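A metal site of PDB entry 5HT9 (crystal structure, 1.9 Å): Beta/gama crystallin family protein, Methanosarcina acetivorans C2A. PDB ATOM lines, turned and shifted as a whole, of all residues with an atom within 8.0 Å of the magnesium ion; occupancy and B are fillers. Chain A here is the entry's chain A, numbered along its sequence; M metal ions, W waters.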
ATOM      1  N   LEU A  31       9.435 -31.116   5.618  1.00  0.00           N
ATOM      2  CA  LEU A  31      10.749 -30.500   5.694  1.00  0.00           C
ATOM      3  C   LEU A  31      11.323 -30.499   7.109  1.00  0.00           C
ATOM      4  O   LEU A  31      12.286 -29.776   7.387  1.00  0.00           O
ATOM      5  CB  LEU A  31      10.690 -29.066   5.147  1.00  0.00           C
ATOM      6  CG  LEU A  31      10.172 -28.909   3.723  1.00  0.00           C
ATOM      7  CD1 LEU A  31      10.435 -27.496   3.187  1.00  0.00           C
ATOM      8  CD2 LEU A  31      10.762 -29.960   2.779  1.00  0.00           C
ATOM      9  N   ASN A  32      10.750 -31.311   8.001  1.00  0.00           N
ATOM     10  CA  ASN A  32      11.329 -31.503   9.329  1.00  0.00           C
ATOM     11  C   ASN A  32      12.794 -31.937   9.211  1.00  0.00           C
ATOM     12  O   ASN A  32      13.085 -32.936   8.545  1.00  0.00           O
ATOM     13  CB  ASN A  32      10.529 -32.526  10.153  1.00  0.00           C
ATOM     14  CG  ASN A  32      11.111 -32.745  11.568  1.00  0.00           C
ATOM     15  OD1 ASN A  32      12.201 -32.273  11.885  1.00  0.00           O
ATOM     16  ND2 ASN A  32      10.383 -33.477  12.392  1.00  0.00           N
ATOM     17  N   ASP A  33      13.683 -31.190   9.853  1.00  0.00           N
ATOM     18  CA  ASP A  33      15.125 -31.459   9.831  1.00  0.00           C
ATOM     19  C   ASP A  33      15.710 -31.429   8.415  1.00  0.00           C
ATOM     20  O   ASP A  33      16.767 -32.001   8.176  1.00  0.00           O
ATOM     21  CB  ASP A  33      15.433 -32.819  10.486  1.00  0.00           C
ATOM     22  CG  ASP A  33      15.724 -32.701  11.983  1.00  0.00           C
ATOM     23  OD1 ASP A  33      15.528 -31.606  12.565  1.00  0.00           O
ATOM     24  OD2 ASP A  33      16.166 -33.721  12.563  1.00  0.00           O
ATOM     25  N   LYS A  34      15.036 -30.758   7.489  1.00  0.00           N
ATOM     26  CA  LYS A  34      15.524 -30.617   6.128  1.00  0.00           C
ATOM     27  C   LYS A  34      15.614 -29.163   5.670  1.00  0.00           C
ATOM     28  O   LYS A  34      16.021 -28.894   4.547  1.00  0.00           O
ATOM     29  CB  LYS A  34      14.636 -31.386   5.152  1.00  0.00           C
ATOM     30  CG  LYS A  34      14.742 -32.892   5.242  1.00  0.00           C
ATOM     31  CD  LYS A  34      13.849 -33.528   4.194  1.00  0.00           C
ATOM     32  CE  LYS A  34      14.013 -35.051   4.174  1.00  0.00           C
ATOM     33  NZ  LYS A  34      13.208 -35.676   3.086  1.00  0.00           N
ATOM     34  N   TYR A  48      12.285 -23.508  15.780  1.00  0.00           N
ATOM     35  CA  TYR A  48      12.724 -24.409  16.848  1.00  0.00           C
ATOM     36  C   TYR A  48      13.403 -25.658  16.313  1.00  0.00           C
ATOM     37  O   TYR A  48      13.051 -26.162  15.248  1.00  0.00           O
ATOM     38  CB  TYR A  48      11.555 -24.867  17.713  1.00  0.00           C
ATOM     39  CG  TYR A  48      10.705 -23.785  18.319  1.00  0.00           C
ATOM     40  CD1 TYR A  48       9.706 -23.168  17.574  1.00  0.00           C
ATOM     41  CD2 TYR A  48      10.852 -23.417  19.646  1.00  0.00           C
ATOM     42  CE1 TYR A  48       8.896 -22.210  18.130  1.00  0.00           C
ATOM     43  CE2 TYR A  48      10.041 -22.446  20.217  1.00  0.00           C
ATOM     44  CZ  TYR A  48       9.065 -21.845  19.449  1.00  0.00           C
ATOM     45  OH  TYR A  48       8.239 -20.895  19.984  1.00  0.00           O
ATOM     46  N   GLU A  49      14.347 -26.204  17.084  1.00  0.00           N
ATOM     47  CA  GLU A  49      15.051 -27.394  16.619  1.00  0.00           C
ATOM     48  C   GLU A  49      14.220 -28.679  16.705  1.00  0.00           C
ATOM     49  O   GLU A  49      14.504 -29.641  15.981  1.00  0.00           O
ATOM     50  CB  GLU A  49      16.371 -27.570  17.381  1.00  0.00           C
ATOM     51  CG  GLU A  49      16.233 -27.775  18.883  1.00  0.00           C
ATOM     52  CD  GLU A  49      17.584 -27.960  19.564  1.00  0.00           C
ATOM     53  OE1 GLU A  49      18.531 -28.438  18.909  1.00  0.00           O
ATOM     54  OE2 GLU A  49      17.686 -27.625  20.757  1.00  0.00           O
ATOM     55  N   TYR A  50      13.206 -28.715  17.559  1.00  0.00           N
ATOM     56  CA  TYR A  50      12.403 -29.939  17.702  1.00  0.00           C
ATOM     57  C   TYR A  50      10.941 -29.666  17.380  1.00  0.00           C
ATOM     58  O   TYR A  50      10.497 -28.515  17.407  1.00  0.00           O
ATOM     59  CB  TYR A  50      12.509 -30.502  19.122  1.00  0.00           C
ATOM     60  CG  TYR A  50      13.917 -30.749  19.586  1.00  0.00           C
ATOM     61  CD1 TYR A  50      14.854 -31.310  18.751  1.00  0.00           C
ATOM     62  CD2 TYR A  50      14.305 -30.395  20.871  1.00  0.00           C
ATOM     63  CE1 TYR A  50      16.143 -31.529  19.168  1.00  0.00           C
ATOM     64  CE2 TYR A  50      15.592 -30.602  21.303  1.00  0.00           C
ATOM     65  CZ  TYR A  50      16.502 -31.170  20.445  1.00  0.00           C
ATOM     66  OH  TYR A  50      17.790 -31.383  20.870  1.00  0.00           O
ATOM     67  N   ILE A  51      10.182 -30.717  17.069  1.00  0.00           N
ATOM     68  CA  ILE A  51       8.767 -30.511  16.755  1.00  0.00           C
ATOM     69  C   ILE A  51       8.013 -30.000  17.964  1.00  0.00           C
ATOM     70  O   ILE A  51       8.485 -30.098  19.098  1.00  0.00           O
ATOM     71  CB  ILE A  51       8.074 -31.776  16.277  1.00  0.00           C
ATOM     72  CG1 ILE A  51       8.198 -32.868  17.343  1.00  0.00           C
ATOM     73  CG2 ILE A  51       8.617 -32.210  14.931  1.00  0.00           C
ATOM     74  CD1 ILE A  51       7.257 -34.010  17.090  1.00  0.00           C
ATOM     75  N   GLY A  54       9.892 -27.232  20.508  1.00  0.00           N
ATOM     76  CA  GLY A  54      10.800 -27.607  21.577  1.00  0.00           C
ATOM     77  C   GLY A  54      12.262 -27.310  21.294  1.00  0.00           C
ATOM     78  O   GLY A  54      12.699 -27.238  20.142  1.00  0.00           O
ATOM     79  N   TRP A  58      15.453 -19.787  17.281  1.00  0.00           N
ATOM     80  CA  TRP A  58      16.039 -18.593  16.711  1.00  0.00           C
ATOM     81  C   TRP A  58      14.937 -17.796  16.053  1.00  0.00           C
ATOM     82  O   TRP A  58      14.074 -18.366  15.411  1.00  0.00           O
ATOM     83  CB  TRP A  58      17.126 -18.963  15.705  1.00  0.00           C
ATOM     84  CG  TRP A  58      18.185 -19.872  16.282  1.00  0.00           C
ATOM     85  CD1 TRP A  58      19.392 -19.496  16.795  1.00  0.00           C
ATOM     86  CD2 TRP A  58      18.106 -21.293  16.413  1.00  0.00           C
ATOM     87  NE1 TRP A  58      20.085 -20.607  17.242  1.00  0.00           N
ATOM     88  CE2 TRP A  58      19.312 -21.724  17.011  1.00  0.00           C
ATOM     89  CE3 TRP A  58      17.138 -22.255  16.086  1.00  0.00           C
ATOM     90  CZ2 TRP A  58      19.572 -23.056  17.285  1.00  0.00           C
ATOM     91  CZ3 TRP A  58      17.411 -23.581  16.357  1.00  0.00           C
ATOM     92  CH2 TRP A  58      18.615 -23.975  16.949  1.00  0.00           C
ATOM     93  N   PRO A  74      21.515 -23.978  12.896  1.00  0.00           N
ATOM     94  CA  PRO A  74      22.086 -25.249  12.394  1.00  0.00           C
ATOM     95  C   PRO A  74      21.343 -25.802  11.174  1.00  0.00           C
ATOM     96  O   PRO A  74      20.113 -25.844  11.190  1.00  0.00           O
ATOM     97  CB  PRO A  74      21.932 -26.187  13.590  1.00  0.00           C
ATOM     98  CG  PRO A  74      21.843 -25.304  14.778  1.00  0.00           C
ATOM     99  CD  PRO A  74      21.141 -24.052  14.318  1.00  0.00           C
ATOM    100  N   ASP A  75      22.068 -26.208  10.150  1.00  0.00           N
ATOM    101  CA  ASP A  75      21.453 -26.741   8.940  1.00  0.00           C
ATOM    102  C   ASP A  75      20.642 -27.991   9.285  1.00  0.00           C
ATOM    103  O   ASP A  75      20.974 -28.699  10.235  1.00  0.00           O
ATOM    104  CB  ASP A  75      22.517 -27.087   7.885  1.00  0.00           C
ATOM    105  CG  ASP A  75      21.922 -27.297   6.500  1.00  0.00           C
ATOM    106  OD1 ASP A  75      20.789 -26.829   6.244  1.00  0.00           O
ATOM    107  OD2 ASP A  75      22.596 -27.913   5.658  1.00  0.00           O
ATOM    108  N   ASN A  76      19.570 -28.230   8.541  1.00  0.00           N
ATOM    109  CA  ASN A  76      18.780 -29.447   8.718  1.00  0.00           C
ATOM    110  C   ASN A  76      18.399 -29.726  10.166  1.00  0.00           C
ATOM    111  O   ASN A  76      18.529 -30.859  10.639  1.00  0.00           O
ATOM    112  CB  ASN A  76      19.564 -30.621   8.130  1.00  0.00           C
ATOM    113  CG  ASN A  76      19.814 -30.459   6.650  1.00  0.00           C
ATOM    114  OD1 ASN A  76      18.983 -29.905   5.935  1.00  0.00           O
ATOM    115  ND2 ASN A  76      20.968 -30.917   6.182  1.00  0.00           N
ATOM    116  N   SER A  77      17.936 -28.694  10.865  1.00  0.00           N
ATOM    117  CA  SER A  77      17.580 -28.800  12.275  1.00  0.00           C
ATOM    118  C   SER A  77      16.178 -28.295  12.601  1.00  0.00           C
ATOM    119  O   SER A  77      15.509 -28.814  13.488  1.00  0.00           O
ATOM    120  CB  SER A  77      18.585 -28.028  13.130  1.00  0.00           C
ATOM    121  OG  SER A  77      19.841 -28.695  13.133  1.00  0.00           O
ATOM    122  N   ILE A  78      15.741 -27.247  11.906  1.00  0.00           N
ATOM    123  CA  ILE A  78      14.431 -26.672  12.183  1.00  0.00           C
ATOM    124  C   ILE A  78      13.332 -27.717  12.003  1.00  0.00           C
ATOM    125  O   ILE A  78      13.245 -28.372  10.973  1.00  0.00           O
ATOM    126  CB  ILE A  78      14.157 -25.460  11.290  1.00  0.00           C
ATOM    127  CG1 ILE A  78      15.195 -24.375  11.573  1.00  0.00           C
ATOM    128  CG2 ILE A  78      12.744 -24.952  11.546  1.00  0.00           C
ATOM    129  CD1 ILE A  78      15.114 -23.186  10.653  1.00  0.00           C
ATOM    130  N   SER A  79      12.516 -27.882  13.037  1.00  0.00           N
ATOM    131  CA  SER A  79      11.515 -28.935  13.070  1.00  0.00           C
ATOM    132  C   SER A  79      10.120 -28.391  13.364  1.00  0.00           C
ATOM    133  O   SER A  79       9.129 -29.113  13.226  1.00  0.00           O
ATOM    134  CB  SER A  79      11.893 -30.004  14.115  1.00  0.00           C
ATOM    135  OG  SER A  79      13.093 -30.671  13.747  1.00  0.00           O
ATOM    136  N   SER A  80      10.039 -27.139  13.800  1.00  0.00           N
ATOM    137  CA  SER A  80       8.764 -26.444  13.890  1.00  0.00           C
ATOM    138  C   SER A  80       9.015 -24.948  13.844  1.00  0.00           C
ATOM    139  O   SER A  80      10.133 -24.493  14.087  1.00  0.00           O
ATOM    140  CB  SER A  80       7.995 -26.829  15.165  1.00  0.00           C
ATOM    141  OG  SER A  80       8.798 -26.639  16.314  1.00  0.00           O
HETATM  142 MG    MG M   1      15.087 -30.665  14.387  1.00  0.00          MG
HETATM  143  O   HOH W   1      14.619 -32.526  15.368  1.00  0.00           O
HETATM  144  O   HOH W   2      17.000 -30.762  15.091  1.00  0.00           O
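OG of Ser 79 sits close to OD1 of Asn 32 (2.6 Å).
N of Ser 79 is in hydrogen-bond range of O of Tyr 48 (2.9 Å).
The side-chain amide oxygen of Asn 32 lies close to the side-chain carboxylate of Asp 33.
N of Asp 33 is in hydrogen-bond range of O of Ile 78 (3.1 Å).
The side-chain hydroxyl (OG) of Ser 77 lies within hydrogen-bond range of the backbone carbonyl oxygen (O) of Asp 75, at 3.1 Å.
The side-chain hydroxyl (OG) of Ser 77 lies close to the backbone carbonyl oxygen (O) of Pro 74, 3.5 Å away.
The magnesium ion is bound by O of Glu 49 (2.0 Å), water W2 (2.0 Å), OG of Ser 79 (2.1 Å), OD1 of Asp 33 (2.1 Å), O of Ser 77 (2.1 Å) and water W1 (2.2 Å).
The magnesium ion has six donor atoms within binding distance.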
